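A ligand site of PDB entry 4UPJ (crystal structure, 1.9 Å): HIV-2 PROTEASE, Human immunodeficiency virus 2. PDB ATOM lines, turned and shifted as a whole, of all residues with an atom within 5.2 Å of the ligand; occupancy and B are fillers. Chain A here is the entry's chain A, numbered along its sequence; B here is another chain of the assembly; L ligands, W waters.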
ATOM      1  N   LEU A  23     -19.698  18.766  22.683  1.00  0.00           N
ATOM      2  CA  LEU A  23     -20.727  19.141  21.743  1.00  0.00           C
ATOM      3  C   LEU A  23     -20.636  18.248  20.504  1.00  0.00           C
ATOM      4  O   LEU A  23     -19.561  18.092  19.938  1.00  0.00           O
ATOM      5  CB  LEU A  23     -20.507  20.601  21.345  1.00  0.00           C
ATOM      6  CG  LEU A  23     -21.432  21.314  20.372  1.00  0.00           C
ATOM      7  CD1 LEU A  23     -22.723  21.635  21.072  1.00  0.00           C
ATOM      8  CD2 LEU A  23     -20.751  22.584  19.892  1.00  0.00           C
ATOM      9  N   ASP A  25     -20.771  17.870  16.962  1.00  0.00           N
ATOM     10  CA  ASP A  25     -20.616  18.805  15.855  1.00  0.00           C
ATOM     11  C   ASP A  25     -20.460  18.142  14.466  1.00  0.00           C
ATOM     12  O   ASP A  25     -19.395  17.660  14.119  1.00  0.00           O
ATOM     13  CB  ASP A  25     -19.373  19.661  16.143  1.00  0.00           C
ATOM     14  CG  ASP A  25     -19.376  21.015  15.450  1.00  0.00           C
ATOM     15  OD1 ASP A  25     -19.526  21.078  14.231  1.00  0.00           O
ATOM     16  OD2 ASP A  25     -19.165  22.024  16.142  1.00  0.00           O
ATOM     17  N   GLY A  27     -20.287  19.664  11.782  1.00  0.00           N
ATOM     18  CA  GLY A  27     -19.514  20.558  10.933  1.00  0.00           C
ATOM     19  C   GLY A  27     -18.013  20.412  11.058  1.00  0.00           C
ATOM     20  O   GLY A  27     -17.264  20.814  10.167  1.00  0.00           O
ATOM     21  N   ALA A  28     -17.560  19.828  12.151  1.00  0.00           N
ATOM     22  CA  ALA A  28     -16.149  19.658  12.397  1.00  0.00           C
ATOM     23  C   ALA A  28     -15.688  18.291  11.934  1.00  0.00           C
ATOM     24  O   ALA A  28     -16.358  17.301  12.141  1.00  0.00           O
ATOM     25  CB  ALA A  28     -15.878  19.823  13.876  1.00  0.00           C
ATOM     26  N   ASP A  29     -14.546  18.262  11.239  1.00  0.00           N
ATOM     27  CA  ASP A  29     -13.967  17.017  10.753  1.00  0.00           C
ATOM     28  C   ASP A  29     -13.245  16.358  11.920  1.00  0.00           C
ATOM     29  O   ASP A  29     -13.167  15.129  11.986  1.00  0.00           O
ATOM     30  CB  ASP A  29     -12.923  17.279   9.650  1.00  0.00           C
ATOM     31  CG  ASP A  29     -13.460  18.115   8.499  1.00  0.00           C
ATOM     32  OD1 ASP A  29     -14.639  18.491   8.483  1.00  0.00           O
ATOM     33  OD2 ASP A  29     -12.676  18.439   7.601  1.00  0.00           O
ATOM     34  N   ASP A  30     -12.739  17.182  12.831  1.00  0.00           N
ATOM     35  CA  ASP A  30     -11.970  16.713  13.967  1.00  0.00           C
ATOM     36  C   ASP A  30     -12.620  16.988  15.297  1.00  0.00           C
ATOM     37  O   ASP A  30     -13.587  17.724  15.378  1.00  0.00           O
ATOM     38  CB  ASP A  30     -10.587  17.361  13.981  1.00  0.00           C
ATOM     39  CG  ASP A  30      -9.887  17.245  12.651  1.00  0.00           C
ATOM     40  OD1 ASP A  30      -9.652  16.108  12.208  1.00  0.00           O
ATOM     41  OD2 ASP A  30      -9.585  18.298  12.038  1.00  0.00           O
ATOM     42  N   ILE A  32     -11.909  18.311  19.218  1.00  0.00           N
ATOM     43  CA  ILE A  32     -10.936  19.019  20.011  1.00  0.00           C
ATOM     44  C   ILE A  32     -11.505  19.368  21.374  1.00  0.00           C
ATOM     45  O   ILE A  32     -12.611  19.878  21.487  1.00  0.00           O
ATOM     46  CB  ILE A  32     -10.389  20.226  19.270  1.00  0.00           C
ATOM     47  CG1 ILE A  32      -9.798  21.182  20.268  1.00  0.00           C
ATOM     48  CG2 ILE A  32     -11.434  20.859  18.407  1.00  0.00           C
ATOM     49  CD1 ILE A  32      -9.021  22.193  19.645  1.00  0.00           C
ATOM     50  N   VAL A  47      -5.529  23.300  13.918  1.00  0.00           N
ATOM     51  CA  VAL A  47      -6.890  23.093  13.500  1.00  0.00           C
ATOM     52  C   VAL A  47      -7.443  24.458  13.193  1.00  0.00           C
ATOM     53  O   VAL A  47      -7.213  25.411  13.929  1.00  0.00           O
ATOM     54  CB  VAL A  47      -7.770  22.296  14.517  1.00  0.00           C
ATOM     55  CG1 VAL A  47      -7.584  22.798  15.920  1.00  0.00           C
ATOM     56  CG2 VAL A  47      -9.219  22.393  14.147  1.00  0.00           C
ATOM     57  N   GLY A  48      -8.023  24.556  12.015  1.00  0.00           N
ATOM     58  CA  GLY A  48      -8.593  25.804  11.571  1.00  0.00           C
ATOM     59  C   GLY A  48     -10.068  25.850  11.845  1.00  0.00           C
ATOM     60  O   GLY A  48     -10.841  25.012  11.398  1.00  0.00           O
ATOM     61  N   GLY A  49     -10.443  26.825  12.651  1.00  0.00           N
ATOM     62  CA  GLY A  49     -11.827  26.993  12.993  1.00  0.00           C
ATOM     63  C   GLY A  49     -12.379  28.064  12.091  1.00  0.00           C
ATOM     64  O   GLY A  49     -11.677  28.589  11.233  1.00  0.00           O
ATOM     65  N   ILE A  50     -13.613  28.438  12.361  1.00  0.00           N
ATOM     66  CA  ILE A  50     -14.310  29.444  11.584  1.00  0.00           C
ATOM     67  C   ILE A  50     -13.698  30.841  11.811  1.00  0.00           C
ATOM     68  O   ILE A  50     -13.778  31.697  10.940  1.00  0.00           O
ATOM     69  CB  ILE A  50     -15.813  29.425  11.946  1.00  0.00           C
ATOM     70  CG1 ILE A  50     -16.619  30.150  10.877  1.00  0.00           C
ATOM     71  CG2 ILE A  50     -16.056  30.100  13.315  1.00  0.00           C
ATOM     72  CD1 ILE A  50     -16.158  29.801   9.494  1.00  0.00           C
ATOM     73  N   GLY A  51     -13.085  31.063  12.965  1.00  0.00           N
ATOM     74  CA  GLY A  51     -12.519  32.368  13.236  1.00  0.00           C
ATOM     75  C   GLY A  51     -11.002  32.463  13.129  1.00  0.00           C
ATOM     76  O   GLY A  51     -10.436  33.561  13.225  1.00  0.00           O
ATOM     77  N   PHE A  53      -7.044  29.866  13.326  1.00  0.00           N
ATOM     78  CA  PHE A  53      -6.364  28.625  13.622  1.00  0.00           C
ATOM     79  C   PHE A  53      -5.788  28.576  15.012  1.00  0.00           C
ATOM     80  O   PHE A  53      -5.252  29.575  15.512  1.00  0.00           O
ATOM     81  CB  PHE A  53      -5.243  28.415  12.594  1.00  0.00           C
ATOM     82  CG  PHE A  53      -5.726  28.270  11.200  1.00  0.00           C
ATOM     83  CD1 PHE A  53      -6.156  29.382  10.492  1.00  0.00           C
ATOM     84  CD2 PHE A  53      -5.856  27.029  10.633  1.00  0.00           C
ATOM     85  CE1 PHE A  53      -6.721  29.257   9.230  1.00  0.00           C
ATOM     86  CE2 PHE A  53      -6.436  26.879   9.369  1.00  0.00           C
ATOM     87  CZ  PHE A  53      -6.858  27.997   8.655  1.00  0.00           C
ATOM     88  N   ILE A  82     -15.201  25.771  23.150  1.00  0.00           N
ATOM     89  CA  ILE A  82     -16.139  24.709  23.545  1.00  0.00           C
ATOM     90  C   ILE A  82     -15.484  23.364  23.204  1.00  0.00           C
ATOM     91  O   ILE A  82     -14.612  23.313  22.335  1.00  0.00           O
ATOM     92  CB  ILE A  82     -17.502  24.781  22.768  1.00  0.00           C
ATOM     93  CG1 ILE A  82     -17.571  25.996  21.863  1.00  0.00           C
ATOM     94  CG2 ILE A  82     -18.661  24.777  23.763  1.00  0.00           C
ATOM     95  CD1 ILE A  82     -18.852  26.048  21.040  1.00  0.00           C
ATOM     96  N   ILE A  84     -15.476  19.934  21.422  1.00  0.00           N
ATOM     97  CA  ILE A  84     -16.172  19.448  20.280  1.00  0.00           C
ATOM     98  C   ILE A  84     -15.799  18.037  19.871  1.00  0.00           C
ATOM     99  O   ILE A  84     -14.636  17.673  19.860  1.00  0.00           O
ATOM    100  CB  ILE A  84     -15.917  20.421  19.093  1.00  0.00           C
ATOM    101  CG1 ILE A  84     -16.711  21.711  19.299  1.00  0.00           C
ATOM    102  CG2 ILE A  84     -16.273  19.775  17.772  1.00  0.00           C
ATOM    103  CD1 ILE A  84     -16.338  22.800  18.346  1.00  0.00           C
ATOM    104  N   ARG B   8     -18.246  15.431   4.783  1.00  0.00           N
ATOM    105  CA  ARG B   8     -18.848  16.643   5.337  1.00  0.00           C
ATOM    106  C   ARG B   8     -20.231  16.860   4.744  1.00  0.00           C
ATOM    107  O   ARG B   8     -20.381  16.840   3.526  1.00  0.00           O
ATOM    108  CB  ARG B   8     -18.030  17.890   4.959  1.00  0.00           C
ATOM    109  CG  ARG B   8     -16.556  17.741   5.015  1.00  0.00           C
ATOM    110  CD  ARG B   8     -15.878  19.018   4.571  1.00  0.00           C
ATOM    111  NE  ARG B   8     -16.167  20.121   5.481  1.00  0.00           N
ATOM    112  CZ  ARG B   8     -15.337  21.121   5.765  1.00  0.00           C
ATOM    113  NH1 ARG B   8     -14.133  21.201   5.214  1.00  0.00           N
ATOM    114  NH2 ARG B   8     -15.688  22.014   6.686  1.00  0.00           N
ATOM    115  N   LEU B  23     -22.559  24.171   4.975  1.00  0.00           N
ATOM    116  CA  LEU B  23     -22.221  23.005   5.777  1.00  0.00           C
ATOM    117  C   LEU B  23     -23.235  22.855   6.905  1.00  0.00           C
ATOM    118  O   LEU B  23     -23.418  23.756   7.714  1.00  0.00           O
ATOM    119  CB  LEU B  23     -20.819  23.157   6.354  1.00  0.00           C
ATOM    120  CG  LEU B  23     -20.246  22.141   7.344  1.00  0.00           C
ATOM    121  CD1 LEU B  23     -20.123  20.772   6.733  1.00  0.00           C
ATOM    122  CD2 LEU B  23     -18.899  22.620   7.765  1.00  0.00           C
ATOM    123  N   ASP B  25     -24.324  22.132  10.200  1.00  0.00           N
ATOM    124  CA  ASP B  25     -23.616  22.083  11.461  1.00  0.00           C
ATOM    125  C   ASP B  25     -24.529  21.938  12.692  1.00  0.00           C
ATOM    126  O   ASP B  25     -25.331  22.830  12.973  1.00  0.00           O
ATOM    127  CB  ASP B  25     -22.778  23.356  11.582  1.00  0.00           C
ATOM    128  CG  ASP B  25     -21.674  23.236  12.580  1.00  0.00           C
ATOM    129  OD1 ASP B  25     -21.865  22.551  13.613  1.00  0.00           O
ATOM    130  OD2 ASP B  25     -20.611  23.817  12.325  1.00  0.00           O
ATOM    131  N   GLY B  27     -23.390  21.620  15.829  1.00  0.00           N
ATOM    132  CA  GLY B  27     -22.778  22.367  16.902  1.00  0.00           C
ATOM    133  C   GLY B  27     -23.108  23.849  16.967  1.00  0.00           C
ATOM    134  O   GLY B  27     -23.169  24.415  18.054  1.00  0.00           O
ATOM    135  N   ALA B  28     -23.380  24.470  15.834  1.00  0.00           N
ATOM    136  CA  ALA B  28     -23.654  25.900  15.817  1.00  0.00           C
ATOM    137  C   ALA B  28     -25.105  26.277  16.117  1.00  0.00           C
ATOM    138  O   ALA B  28     -26.036  25.574  15.742  1.00  0.00           O
ATOM    139  CB  ALA B  28     -23.218  26.482  14.492  1.00  0.00           C
ATOM    140  N   GLY B  48     -18.721  34.116  18.242  1.00  0.00           N
ATOM    141  CA  GLY B  48     -17.451  33.554  18.657  1.00  0.00           C
ATOM    142  C   GLY B  48     -17.319  32.103  18.251  1.00  0.00           C
ATOM    143  O   GLY B  48     -18.178  31.289  18.579  1.00  0.00           O
ATOM    144  N   GLY B  49     -16.282  31.781  17.484  1.00  0.00           N
ATOM    145  CA  GLY B  49     -16.080  30.406  17.064  1.00  0.00           C
ATOM    146  C   GLY B  49     -14.712  29.934  17.477  1.00  0.00           C
ATOM    147  O   GLY B  49     -14.096  30.542  18.333  1.00  0.00           O
ATOM    148  N   ILE B  50     -14.243  28.806  16.947  1.00  0.00           N
ATOM    149  CA  ILE B  50     -12.907  28.334  17.304  1.00  0.00           C
ATOM    150  C   ILE B  50     -12.024  29.257  16.503  1.00  0.00           C
ATOM    151  O   ILE B  50     -12.326  29.553  15.340  1.00  0.00           O
ATOM    152  CB  ILE B  50     -12.639  26.876  16.821  1.00  0.00           C
ATOM    153  CG1 ILE B  50     -13.732  25.931  17.309  1.00  0.00           C
ATOM    154  CG2 ILE B  50     -11.265  26.395  17.303  1.00  0.00           C
ATOM    155  CD1 ILE B  50     -13.879  25.830  18.799  1.00  0.00           C
ATOM    156  N   PRO B  81     -14.858  31.789   6.026  1.00  0.00           N
ATOM    157  CA  PRO B  81     -14.265  30.884   5.024  1.00  0.00           C
ATOM    158  C   PRO B  81     -15.202  29.740   4.654  1.00  0.00           C
ATOM    159  O   PRO B  81     -15.030  29.086   3.622  1.00  0.00           O
ATOM    160  CB  PRO B  81     -13.048  30.326   5.748  1.00  0.00           C
ATOM    161  CG  PRO B  81     -13.453  30.373   7.202  1.00  0.00           C
ATOM    162  CD  PRO B  81     -14.108  31.730   7.295  1.00  0.00           C
ATOM    163  N   ILE B  82     -16.204  29.517   5.490  1.00  0.00           N
ATOM    164  CA  ILE B  82     -17.122  28.425   5.254  1.00  0.00           C
ATOM    165  C   ILE B  82     -18.535  28.817   5.682  1.00  0.00           C
ATOM    166  O   ILE B  82     -18.725  29.388   6.745  1.00  0.00           O
ATOM    167  CB  ILE B  82     -16.594  27.154   5.962  1.00  0.00           C
ATOM    168  CG1 ILE B  82     -17.383  25.925   5.568  1.00  0.00           C
ATOM    169  CG2 ILE B  82     -16.604  27.309   7.474  1.00  0.00           C
ATOM    170  CD1 ILE B  82     -16.615  24.678   5.908  1.00  0.00           C
ATOM    171  N   ILE B  84     -22.035  28.179   7.019  1.00  0.00           N
ATOM    172  CA  ILE B  84     -22.560  27.230   7.951  1.00  0.00           C
ATOM    173  C   ILE B  84     -24.029  27.457   8.208  1.00  0.00           C
ATOM    174  O   ILE B  84     -24.457  28.592   8.374  1.00  0.00           O
ATOM    175  CB  ILE B  84     -21.818  27.369   9.288  1.00  0.00           C
ATOM    176  CG1 ILE B  84     -20.357  27.017   9.107  1.00  0.00           C
ATOM    177  CG2 ILE B  84     -22.439  26.466  10.339  1.00  0.00           C
ATOM    178  CD1 ILE B  84     -19.514  27.535  10.219  1.00  0.00           C
HETATM  179  C1  LIG L   1     -16.897  25.242  14.111  1.00  0.00           C
HETATM  180  C2  LIG L   1     -16.163  26.396  14.516  1.00  0.00           C
HETATM  181  C3  LIG L   1     -17.781  26.854  16.156  1.00  0.00           C
HETATM  182  C4  LIG L   1     -18.233  27.676  17.235  1.00  0.00           C
HETATM  183  C5  LIG L   1     -19.419  27.355  17.897  1.00  0.00           C
HETATM  184  C6  LIG L   1     -20.172  26.235  17.515  1.00  0.00           C
HETATM  185  C7  LIG L   1     -19.748  25.410  16.456  1.00  0.00           C
HETATM  186  C8  LIG L   1     -18.548  25.734  15.776  1.00  0.00           C
HETATM  187  C9  LIG L   1     -18.093  24.914  14.738  1.00  0.00           C
HETATM  188  C10 LIG L   1     -16.340  24.253  13.100  1.00  0.00           C
HETATM  189  C11 LIG L   1     -15.152  23.473  13.639  1.00  0.00           C
HETATM  190  C12 LIG L   1     -15.133  23.008  14.977  1.00  0.00           C
HETATM  191  C13 LIG L   1     -14.009  22.257  15.431  1.00  0.00           C
HETATM  192  C14 LIG L   1     -12.931  21.960  14.559  1.00  0.00           C
HETATM  193  C15 LIG L   1     -12.978  22.425  13.223  1.00  0.00           C
HETATM  194  C16 LIG L   1     -14.079  23.177  12.796  1.00  0.00           C
HETATM  195  C17 LIG L   1     -16.124  24.849  11.690  1.00  0.00           C
HETATM  196  C18 LIG L   1     -17.437  25.155  11.010  1.00  0.00           C
HETATM  197  C19 LIG L   1     -12.399  21.152  11.442  1.00  0.00           C
HETATM  198  C20 LIG L   1     -12.781  21.560  10.003  1.00  0.00           C
HETATM  199  C21 LIG L   1     -12.201  23.358   8.387  1.00  0.00           C
HETATM  200  C22 LIG L   1     -11.756  25.730   7.812  1.00  0.00           C
HETATM  201  C23 LIG L   1     -12.807  26.318   8.750  1.00  0.00           C
HETATM  202  C24 LIG L   1     -10.602  26.723   7.799  1.00  0.00           C
HETATM  203  C25 LIG L   1     -12.357  25.716   6.375  1.00  0.00           C
HETATM  204  N1  LIG L   1     -12.038  22.164  12.221  1.00  0.00           N
HETATM  205  N2  LIG L   1     -11.904  22.636   9.480  1.00  0.00           N
HETATM  206  O1  LIG L   1     -15.146  26.710  13.949  1.00  0.00           O
HETATM  207  O2  LIG L   1     -16.571  27.216  15.521  1.00  0.00           O
HETATM  208  O3  LIG L   1     -18.781  23.818  14.296  1.00  0.00           O
HETATM  209  O4  LIG L   1     -12.459  20.019  11.813  1.00  0.00           O
HETATM  210  O5  LIG L   1     -13.095  23.138   7.606  1.00  0.00           O
HETATM  211  O6  LIG L   1     -11.315  24.414   8.223  1.00  0.00           O
HETATM  212  O   HOH W   1      -8.582  22.478  10.265  1.00  0.00           O
HETATM  213  O   HOH W   2      -9.724  29.510   9.641  1.00  0.00           O
HETATM  214  O   HOH W   3      -9.746  20.121  10.042  1.00  0.00           O
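The side-chain carboxylate of Asp 25 of chain A lies within hydrogen-bond range of an oxygen (O3) of the ligand, at 2.6 Å. O3 of the ligand is in hydrogen-bond range of OD2 of Asp 25 of chain B, at 2.7 Å. N of Asp 29 sits at hydrogen-bond distance from O4 of the ligand (2.8 Å). The backbone NH (N) of Ile 50 of chain A lies within hydrogen-bond range of an oxygen (O1) of the ligand (2.8 Å). NH2 of Arg 8 of chain B lies within hydrogen-bond range of O5 of the ligand. N of Asp 30 lies within hydrogen-bond range of O4 of the ligand. The backbone NH (N) of Ile 50 of chain B lies within hydrogen-bond range of an oxygen (O2) of the ligand, 3.2 Å away. A nitrogen (N1) of the ligand is in hydrogen-bond range of the backbone carbonyl oxygen of Gly 48 of chain A (3.2 Å).
The side-chain carboxylate (OD1) of Asp 25 of chain A sits at hydrogen-bond distance from the backbone NH (N) of Ala 28 of chain A (3.1 Å). The backbone NH (N) of Gly 27 of chain A lies within hydrogen-bond range of the side-chain carboxylate (OD1) of Asp 25 of chain A (2.9 Å). The side-chain carboxylate (OD1) of Asp 25 of chain B is in hydrogen-bond range of the backbone NH (N) of Gly 27 of chain B, at 2.8 Å. OD1 of Asp 25 of chain B is in hydrogen-bond range of N of Ala 28 of chain B. OD1 of Asp 29 is in salt-bridge range of NE of Arg 8 of chain B, at 3.7 Å. The backbone NH of Ile 50 of chain A is in hydrogen-bond range of the backbone carbonyl oxygen of Ile 50 of chain B. O of Ile 50 of chain B sits at hydrogen-bond distance from N of Gly 51 (2.9 Å). N of Ile 84 of chain A lies within hydrogen-bond range of O of Ile 32.
Ala 28 of chain A touches the ligand (CB to C13, 3.4 Å). Val 47 touches the ligand. CA of Gly 49 of chain A touches O1 of the ligand (3.5 Å). Ile 82 of chain A touches the ligand (CD1 to C5, 3.5 Å). Ile 84 of chain A touches the ligand. Gly 27 of chain B touches the ligand. Ala 28 of chain B touches the ligand. Gly 48 of chain B touches the ligand. Gly 49 of chain B touches the ligand (CA to C4, 3.5 Å). CD1 of Ile 84 of chain B touches C18 of the ligand, 3.3 Å away. Of the 26 residues printed, 18 come within 4 Å of the ligand.
Water W3 bridges the side-chain carboxylate (OD2) of Asp 30 (2.7 Å) and an oxygen (O4) of the ligand (3.2 Å). Water W1 lies within hydrogen-bond range of N of Gly 48 of chain A (2.8 Å) and N2 of the ligand (3.4 Å).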
